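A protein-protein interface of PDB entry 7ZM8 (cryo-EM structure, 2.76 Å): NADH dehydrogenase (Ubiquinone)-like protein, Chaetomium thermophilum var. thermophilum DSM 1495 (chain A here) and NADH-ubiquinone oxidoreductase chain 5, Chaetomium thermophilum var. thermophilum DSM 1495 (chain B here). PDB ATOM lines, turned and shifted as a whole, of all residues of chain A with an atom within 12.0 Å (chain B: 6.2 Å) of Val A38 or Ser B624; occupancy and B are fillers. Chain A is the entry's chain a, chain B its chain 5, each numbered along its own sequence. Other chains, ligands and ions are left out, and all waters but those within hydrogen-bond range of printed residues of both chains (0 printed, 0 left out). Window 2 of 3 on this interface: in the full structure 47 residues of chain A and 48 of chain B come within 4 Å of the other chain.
N of Phe A32 is in hydrogen-bond range of O of Ser B626 (2.8 Å).
OG of Ser B626 is in hydrogen-bond range of N of Leu A33 (3.0 Å).
NH1 of Arg A40 sits close to OG of Ser B622, at 3.4 Å.
The guanidinium group (NE) of Arg A40 is in salt-bridge range of the side-chain carboxylate (OD1) of Asp A44 (3.8 Å).
O of Asn B619 is in hydrogen-bond range of OG of Ser B622, at 2.6 Å.
The backbone carbonyl oxygen (O) of Ser B621 is in hydrogen-bond range of the side-chain hydroxyl (OG) of Ser B624 (2.8 Å).
The side-chain hydroxyl of Tyr B631 lies within hydrogen-bond range of the backbone NH of Ser B626.
O of Val A38 touches O of Ser B624, at 3.7 Å.
CG2 of Val A38 touches OG of Ser B626, 3.9 Å away.
Asn B619 touches Arg A40.
Of the printed residues of chain B, Phe A32 touches Ser B626.
Of the printed residues of chain B, Leu A33 touches Ser B626 (3.0 Å).
Of chain B, only Ser B624 (3.7 Å) and Ser B626 (3.9 Å) come within 4 Å of Val A38.
Printed residues of chain B within 4 Å of Arg A40: Asn B619 (3.5 Å) and Ser B622 (3.2 Å).
Printed residues of chain A within 4 Å of Asn B619: Arg A40 (3.5 Å).
Ser B622 touches one residue of chain A.
No residue of chain A comes within 4 Å of Leu B623.
Of chain A, only Val A38 (3.7 Å) comes within 4 Å of Ser B624.
No residue of chain A comes within 4 Å of Thr B625.
Ser B626 touches just these residues of chain A: Phe A32 (2.8 Å), Leu A33 (3.0 Å) and Val A38 (3.9 Å).
No residue of chain A comes within 4 Å of His B627.
Tyr B631 touches none of the printed residues of chain A.
The nearest residue of chain B that does not touch Val A38 is Thr B625 (4.4 Å).
The nearest printed residue of chain B that does not touch Phe A32 is His B627 (4.1 Å).
Along chain A the printed residues that touch a printed residue of chain B span positions 32 to 40.
Of the 11 printed residues of chain B, 4 touch a printed residue of chain A.
Printed residues of chain B that touch a printed residue of chain A: Asn B619, Ser B622, Ser B624 and Ser B626.
Among the printed residues, 6 pairs touch across the chains.
Among the printed residues, no Asp or Glu carboxylate lies within 4 Å of a Lys or Arg side-chain nitrogen of the other chain.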
ATOM      1  N   PHE A  32       8.048  13.497 -19.347  1.00  0.00           N
ATOM      2  CA  PHE A  32       7.556  13.946 -18.019  1.00  0.00           C
ATOM      3  C   PHE A  32       8.669  13.811 -16.979  1.00  0.00           C
ATOM      4  O   PHE A  32       8.668  14.572 -16.001  1.00  0.00           O
ATOM      5  CB  PHE A  32       6.238  13.266 -17.642  1.00  0.00           C
ATOM      6  CG  PHE A  32       5.007  14.000 -18.107  1.00  0.00           C
ATOM      7  CD1 PHE A  32       5.053  15.361 -18.367  1.00  0.00           C
ATOM      8  CD2 PHE A  32       3.804  13.336 -18.281  1.00  0.00           C
ATOM      9  CE1 PHE A  32       3.924  16.041 -18.794  1.00  0.00           C
ATOM     10  CE2 PHE A  32       2.677  14.018 -18.711  1.00  0.00           C
ATOM     11  CZ  PHE A  32       2.737  15.367 -18.961  1.00  0.00           C
ATOM     12  N   LEU A  33       9.585  12.863 -17.183  1.00  0.00           N
ATOM     13  CA  LEU A  33      10.620  12.604 -16.154  1.00  0.00           C
ATOM     14  C   LEU A  33      11.909  13.399 -16.429  1.00  0.00           C
ATOM     15  O   LEU A  33      12.055  13.868 -17.562  1.00  0.00           O
ATOM     16  CB  LEU A  33      10.872  11.102 -16.032  1.00  0.00           C
ATOM     17  CG  LEU A  33       9.744  10.302 -15.387  1.00  0.00           C
ATOM     18  CD1 LEU A  33       9.956   8.812 -15.585  1.00  0.00           C
ATOM     19  CD2 LEU A  33       9.629  10.632 -13.910  1.00  0.00           C
ATOM     20  N   PRO A  34      12.835  13.600 -15.450  1.00  0.00           N
ATOM     21  CA  PRO A  34      14.091  14.304 -15.715  1.00  0.00           C
ATOM     22  C   PRO A  34      14.966  13.549 -16.696  1.00  0.00           C
ATOM     23  O   PRO A  34      14.891  12.326 -16.821  1.00  0.00           O
ATOM     24  CB  PRO A  34      14.754  14.380 -14.336  1.00  0.00           C
ATOM     25  CG  PRO A  34      13.660  14.151 -13.370  1.00  0.00           C
ATOM     26  CD  PRO A  34      12.704  13.236 -14.030  1.00  0.00           C
ATOM     27  N   GLU A  35      15.804  14.305 -17.407  1.00  0.00           N
ATOM     28  CA  GLU A  35      16.758  13.703 -18.329  1.00  0.00           C
ATOM     29  C   GLU A  35      17.845  12.926 -17.605  1.00  0.00           C
ATOM     30  O   GLU A  35      18.456  12.037 -18.200  1.00  0.00           O
ATOM     31  CB  GLU A  35      17.387  14.782 -19.210  1.00  0.00           C
ATOM     32  CG  GLU A  35      16.438  15.365 -20.244  1.00  0.00           C
ATOM     33  CD  GLU A  35      16.093  14.374 -21.337  1.00  0.00           C
ATOM     34  OE1 GLU A  35      16.968  13.561 -21.700  1.00  0.00           O
ATOM     35  OE2 GLU A  35      14.947  14.406 -21.833  1.00  0.00           O
ATOM     36  N   ALA A  36      18.098  13.245 -16.338  1.00  0.00           N
ATOM     37  CA  ALA A  36      19.064  12.502 -15.546  1.00  0.00           C
ATOM     38  C   ALA A  36      18.616  11.078 -15.268  1.00  0.00           C
ATOM     39  O   ALA A  36      19.451  10.231 -14.944  1.00  0.00           O
ATOM     40  CB  ALA A  36      19.313  13.229 -14.226  1.00  0.00           C
ATOM     41  N   MET A  37      17.320  10.798 -15.382  1.00  0.00           N
ATOM     42  CA  MET A  37      16.759   9.513 -15.000  1.00  0.00           C
ATOM     43  C   MET A  37      16.408   8.616 -16.172  1.00  0.00           C
ATOM     44  O   MET A  37      16.486   7.394 -16.035  1.00  0.00           O
ATOM     45  CB  MET A  37      15.499   9.724 -14.153  1.00  0.00           C
ATOM     46  CG  MET A  37      15.759  10.354 -12.803  1.00  0.00           C
ATOM     47  SD  MET A  37      14.248  10.657 -11.888  1.00  0.00           S
ATOM     48  CE  MET A  37      13.733   9.001 -11.463  1.00  0.00           C
ATOM     49  N   VAL A  38      16.018   9.176 -17.313  1.00  0.00           N
ATOM     50  CA  VAL A  38      15.577   8.367 -18.444  1.00  0.00           C
ATOM     51  C   VAL A  38      16.321   8.786 -19.703  1.00  0.00           C
ATOM     52  O   VAL A  38      16.257   8.101 -20.728  1.00  0.00           O
ATOM     53  CB  VAL A  38      14.052   8.472 -18.653  1.00  0.00           C
ATOM     54  CG1 VAL A  38      13.312   8.179 -17.371  1.00  0.00           C
ATOM     55  CG2 VAL A  38      13.677   9.851 -19.173  1.00  0.00           C
ATOM     56  N   GLY A  39      17.031   9.907 -19.637  1.00  0.00           N
ATOM     57  CA  GLY A  39      17.690  10.425 -20.820  1.00  0.00           C
ATOM     58  C   GLY A  39      18.795   9.514 -21.323  1.00  0.00           C
ATOM     59  O   GLY A  39      19.493   8.854 -20.555  1.00  0.00           O
ATOM     60  N   ARG A  40      18.944   9.477 -22.649  1.00  0.00           N
ATOM     61  CA  ARG A  40      20.054   8.753 -23.257  1.00  0.00           C
ATOM     62  C   ARG A  40      21.392   9.402 -22.937  1.00  0.00           C
ATOM     63  O   ARG A  40      22.425   8.726 -22.988  1.00  0.00           O
ATOM     64  CB  ARG A  40      19.869   8.674 -24.778  1.00  0.00           C
ATOM     65  CG  ARG A  40      20.947   7.865 -25.494  1.00  0.00           C
ATOM     66  CD  ARG A  40      20.958   8.091 -26.998  1.00  0.00           C
ATOM     67  NE  ARG A  40      22.097   7.423 -27.626  1.00  0.00           N
ATOM     68  CZ  ARG A  40      22.065   6.189 -28.123  1.00  0.00           C
ATOM     69  NH1 ARG A  40      20.943   5.494 -28.086  1.00  0.00           N
ATOM     70  NH2 ARG A  40      23.147   5.658 -28.670  1.00  0.00           N
ATOM     71  N   SER A  41      21.389  10.688 -22.588  1.00  0.00           N
ATOM     72  CA  SER A  41      22.635  11.422 -22.412  1.00  0.00           C
ATOM     73  C   SER A  41      23.487  10.827 -21.302  1.00  0.00           C
ATOM     74  O   SER A  41      24.715  10.756 -21.424  1.00  0.00           O
ATOM     75  CB  SER A  41      22.335  12.893 -22.124  1.00  0.00           C
ATOM     76  OG  SER A  41      23.523  13.609 -21.839  1.00  0.00           O
ATOM     77  N   LYS A  42      22.865  10.401 -20.206  1.00  0.00           N
ATOM     78  CA  LYS A  42      23.648   9.885 -19.094  1.00  0.00           C
ATOM     79  C   LYS A  42      23.949   8.402 -19.249  1.00  0.00           C
ATOM     80  O   LYS A  42      24.811   7.877 -18.538  1.00  0.00           O
ATOM     81  CB  LYS A  42      22.932  10.193 -17.771  1.00  0.00           C
ATOM     82  CG  LYS A  42      23.714   9.829 -16.528  1.00  0.00           C
ATOM     83  CD  LYS A  42      22.934  10.105 -15.272  1.00  0.00           C
ATOM     84  CE  LYS A  42      22.861  11.595 -14.996  1.00  0.00           C
ATOM     85  NZ  LYS A  42      22.197  11.884 -13.697  1.00  0.00           N
ATOM     86  N   ILE A  43      23.277   7.721 -20.176  1.00  0.00           N
ATOM     87  CA  ILE A  43      23.763   6.420 -20.623  1.00  0.00           C
ATOM     88  C   ILE A  43      25.104   6.583 -21.325  1.00  0.00           C
ATOM     89  O   ILE A  43      26.044   5.815 -21.096  1.00  0.00           O
ATOM     90  CB  ILE A  43      22.729   5.743 -21.537  1.00  0.00           C
ATOM     91  CG1 ILE A  43      21.401   5.557 -20.803  1.00  0.00           C
ATOM     92  CG2 ILE A  43      23.245   4.403 -22.000  1.00  0.00           C
ATOM     93  CD1 ILE A  43      21.490   4.687 -19.588  1.00  0.00           C
ATOM     94  N   ASP A  44      25.220   7.609 -22.167  1.00  0.00           N
ATOM     95  CA  ASP A  44      26.440   7.878 -22.912  1.00  0.00           C
ATOM     96  C   ASP A  44      27.616   8.259 -22.024  1.00  0.00           C
ATOM     97  O   ASP A  44      28.751   8.264 -22.504  1.00  0.00           O
ATOM     98  CB  ASP A  44      26.182   8.985 -23.932  1.00  0.00           C
ATOM     99  CG  ASP A  44      25.526   8.467 -25.194  1.00  0.00           C
ATOM    100  OD1 ASP A  44      24.926   7.373 -25.147  1.00  0.00           O
ATOM    101  OD2 ASP A  44      25.609   9.154 -26.236  1.00  0.00           O
ATOM    102  N   GLU A  45      27.378   8.595 -20.758  1.00  0.00           N
ATOM    103  CA  GLU A  45      28.467   8.804 -19.815  1.00  0.00           C
ATOM    104  C   GLU A  45      28.839   7.517 -19.093  1.00  0.00           C
ATOM    105  O   GLU A  45      30.016   7.284 -18.803  1.00  0.00           O
ATOM    106  CB  GLU A  45      28.086   9.881 -18.798  1.00  0.00           C
ATOM    107  CG  GLU A  45      29.274  10.522 -18.094  1.00  0.00           C
ATOM    108  CD  GLU A  45      28.931  11.862 -17.473  1.00  0.00           C
ATOM    109  OE1 GLU A  45      28.128  12.608 -18.069  1.00  0.00           O
ATOM    110  OE2 GLU A  45      29.462  12.165 -16.384  1.00  0.00           O
ATOM    111  N   LYS A  46      27.850   6.678 -18.795  1.00  0.00           N
ATOM    112  CA  LYS A  46      28.128   5.400 -18.153  1.00  0.00           C
ATOM    113  C   LYS A  46      28.725   4.414 -19.148  1.00  0.00           C
ATOM    114  O   LYS A  46      29.588   3.605 -18.792  1.00  0.00           O
ATOM    115  CB  LYS A  46      26.843   4.824 -17.566  1.00  0.00           C
ATOM    116  CG  LYS A  46      26.171   5.684 -16.531  1.00  0.00           C
ATOM    117  CD  LYS A  46      26.990   5.847 -15.277  1.00  0.00           C
ATOM    118  CE  LYS A  46      26.174   6.578 -14.230  1.00  0.00           C
ATOM    119  NZ  LYS A  46      25.948   7.993 -14.624  1.00  0.00           N
ATOM    120  N   TYR A  47      28.262   4.461 -20.392  1.00  0.00           N
ATOM    121  CA  TYR A  47      28.657   3.519 -21.434  1.00  0.00           C
ATOM    122  C   TYR A  47      29.035   4.296 -22.687  1.00  0.00           C
ATOM    123  O   TYR A  47      28.369   4.188 -23.723  1.00  0.00           O
ATOM    124  CB  TYR A  47      27.528   2.528 -21.718  1.00  0.00           C
ATOM    125  CG  TYR A  47      27.096   1.740 -20.504  1.00  0.00           C
ATOM    126  CD1 TYR A  47      27.753   0.574 -20.145  1.00  0.00           C
ATOM    127  CD2 TYR A  47      26.040   2.165 -19.711  1.00  0.00           C
ATOM    128  CE1 TYR A  47      27.372  -0.144 -19.041  1.00  0.00           C
ATOM    129  CE2 TYR A  47      25.652   1.452 -18.602  1.00  0.00           C
ATOM    130  CZ  TYR A  47      26.322   0.297 -18.272  1.00  0.00           C
ATOM    131  OH  TYR A  47      25.944  -0.430 -17.166  1.00  0.00           O
ATOM    132  N   ASN B 619      20.495   1.953 -28.180  1.00  0.00           N
ATOM    133  CA  ASN B 619      19.534   2.450 -29.153  1.00  0.00           C
ATOM    134  C   ASN B 619      18.104   2.148 -28.724  1.00  0.00           C
ATOM    135  O   ASN B 619      17.232   3.021 -28.782  1.00  0.00           O
ATOM    136  CB  ASN B 619      19.830   1.846 -30.521  1.00  0.00           C
ATOM    137  CG  ASN B 619      21.157   2.308 -31.083  1.00  0.00           C
ATOM    138  OD1 ASN B 619      21.480   3.491 -31.045  1.00  0.00           O
ATOM    139  ND2 ASN B 619      21.940   1.373 -31.600  1.00  0.00           N
ATOM    140  N   ILE B 620      17.839   0.911 -28.300  1.00  0.00           N
ATOM    141  CA  ILE B 620      16.506   0.570 -27.815  1.00  0.00           C
ATOM    142  C   ILE B 620      16.180   1.373 -26.566  1.00  0.00           C
ATOM    143  O   ILE B 620      15.049   1.831 -26.380  1.00  0.00           O
ATOM    144  CB  ILE B 620      16.391  -0.943 -27.555  1.00  0.00           C
ATOM    145  CG1 ILE B 620      16.833  -1.742 -28.775  1.00  0.00           C
ATOM    146  CG2 ILE B 620      14.974  -1.313 -27.182  1.00  0.00           C
ATOM    147  CD1 ILE B 620      16.975  -3.215 -28.505  1.00  0.00           C
ATOM    148  N   SER B 621      17.166   1.549 -25.686  1.00  0.00           N
ATOM    149  CA  SER B 621      16.954   2.331 -24.479  1.00  0.00           C
ATOM    150  C   SER B 621      16.703   3.800 -24.780  1.00  0.00           C
ATOM    151  O   SER B 621      16.175   4.513 -23.925  1.00  0.00           O
ATOM    152  CB  SER B 621      18.154   2.186 -23.548  1.00  0.00           C
ATOM    153  OG  SER B 621      17.986   2.963 -22.380  1.00  0.00           O
ATOM    154  N   SER B 622      17.065   4.264 -25.972  1.00  0.00           N
ATOM    155  CA  SER B 622      16.786   5.631 -26.381  1.00  0.00           C
ATOM    156  C   SER B 622      15.396   5.798 -26.974  1.00  0.00           C
ATOM    157  O   SER B 622      15.025   6.920 -27.332  1.00  0.00           O
ATOM    158  CB  SER B 622      17.836   6.099 -27.388  1.00  0.00           C
ATOM    159  OG  SER B 622      17.590   5.554 -28.670  1.00  0.00           O
ATOM    160  N   LEU B 623      14.628   4.715 -27.099  1.00  0.00           N
ATOM    161  CA  LEU B 623      13.230   4.837 -27.488  1.00  0.00           C
ATOM    162  C   LEU B 623      12.359   5.270 -26.318  1.00  0.00           C
ATOM    163  O   LEU B 623      11.210   5.673 -26.521  1.00  0.00           O
ATOM    164  CB  LEU B 623      12.721   3.513 -28.052  1.00  0.00           C
ATOM    165  CG  LEU B 623      13.282   3.056 -29.395  1.00  0.00           C
ATOM    166  CD1 LEU B 623      13.037   1.572 -29.593  1.00  0.00           C
ATOM    167  CD2 LEU B 623      12.666   3.854 -30.522  1.00  0.00           C
ATOM    168  N   SER B 624      12.879   5.191 -25.097  1.00  0.00           N
ATOM    169  CA  SER B 624      12.091   5.422 -23.888  1.00  0.00           C
ATOM    170  C   SER B 624      12.323   6.844 -23.406  1.00  0.00           C
ATOM    171  O   SER B 624      13.249   7.106 -22.636  1.00  0.00           O
ATOM    172  CB  SER B 624      12.463   4.410 -22.813  1.00  0.00           C
ATOM    173  OG  SER B 624      13.798   4.609 -22.386  1.00  0.00           O
ATOM    174  N   THR B 625      11.468   7.766 -23.837  1.00  0.00           N
ATOM    175  CA  THR B 625      11.635   9.179 -23.540  1.00  0.00           C
ATOM    176  C   THR B 625      10.710   9.667 -22.434  1.00  0.00           C
ATOM    177  O   THR B 625      10.669  10.869 -22.162  1.00  0.00           O
ATOM    178  CB  THR B 625      11.425  10.003 -24.807  1.00  0.00           C
ATOM    179  OG1 THR B 625      10.092   9.803 -25.290  1.00  0.00           O
ATOM    180  CG2 THR B 625      12.411   9.576 -25.879  1.00  0.00           C
ATOM    181  N   SER B 626       9.986   8.756 -21.781  1.00  0.00           N
ATOM    182  CA  SER B 626       9.039   9.082 -20.716  1.00  0.00           C
ATOM    183  C   SER B 626       8.007  10.112 -21.165  1.00  0.00           C
ATOM    184  O   SER B 626       7.589  10.969 -20.384  1.00  0.00           O
ATOM    185  CB  SER B 626       9.755   9.565 -19.454  1.00  0.00           C
ATOM    186  OG  SER B 626       9.967  10.963 -19.488  1.00  0.00           O
ATOM    187  N   HIS B 627       7.593  10.048 -22.426  1.00  0.00           N
ATOM    188  CA  HIS B 627       6.469  10.829 -22.915  1.00  0.00           C
ATOM    189  C   HIS B 627       5.269   9.905 -23.028  1.00  0.00           C
ATOM    190  O   HIS B 627       5.331   8.885 -23.718  1.00  0.00           O
ATOM    191  CB  HIS B 627       6.768  11.479 -24.263  1.00  0.00           C
ATOM    192  CG  HIS B 627       7.971  12.362 -24.252  1.00  0.00           C
ATOM    193  ND1 HIS B 627       9.001  12.226 -25.156  1.00  0.00           N
ATOM    194  CD2 HIS B 627       8.314  13.389 -23.441  1.00  0.00           C
ATOM    195  CE1 HIS B 627       9.925  13.133 -24.904  1.00  0.00           C
ATOM    196  NE2 HIS B 627       9.535  13.851 -23.867  1.00  0.00           N
ATOM    197  N   TYR B 631       4.477   6.943 -25.725  1.00  0.00           N
ATOM    198  CA  TYR B 631       4.256   5.583 -25.247  1.00  0.00           C
ATOM    199  C   TYR B 631       2.910   5.055 -25.712  1.00  0.00           C
ATOM    200  O   TYR B 631       2.774   3.867 -26.021  1.00  0.00           O
ATOM    201  CB  TYR B 631       4.343   5.535 -23.722  1.00  0.00           C
ATOM    202  CG  TYR B 631       5.745   5.593 -23.169  1.00  0.00           C
ATOM    203  CD1 TYR B 631       6.847   5.525 -24.003  1.00  0.00           C
ATOM    204  CD2 TYR B 631       5.963   5.719 -21.809  1.00  0.00           C
ATOM    205  CE1 TYR B 631       8.128   5.582 -23.495  1.00  0.00           C
ATOM    206  CE2 TYR B 631       7.237   5.778 -21.295  1.00  0.00           C
ATOM    207  CZ  TYR B 631       8.315   5.708 -22.142  1.00  0.00           C
ATOM    208  OH  TYR B 631       9.582   5.768 -21.621  1.00  0.00           O
ATOM    209  N   TYR B 634       3.158   3.736 -29.138  1.00  0.00           N
ATOM    210  CA  TYR B 634       3.806   2.430 -29.169  1.00  0.00           C
ATOM    211  C   TYR B 634       2.818   1.309 -28.879  1.00  0.00           C
ATOM    212  O   TYR B 634       2.864   0.254 -29.518  1.00  0.00           O
ATOM    213  CB  TYR B 634       4.956   2.390 -28.164  1.00  0.00           C
ATOM    214  CG  TYR B 634       6.141   3.248 -28.522  1.00  0.00           C
ATOM    215  CD1 TYR B 634       6.288   3.766 -29.798  1.00  0.00           C
ATOM    216  CD2 TYR B 634       7.116   3.537 -27.583  1.00  0.00           C
ATOM    217  CE1 TYR B 634       7.373   4.548 -30.128  1.00  0.00           C
ATOM    218  CE2 TYR B 634       8.208   4.318 -27.904  1.00  0.00           C
ATOM    219  CZ  TYR B 634       8.330   4.819 -29.179  1.00  0.00           C
ATOM    220  OH  TYR B 634       9.407   5.602 -29.510  1.00  0.00           O
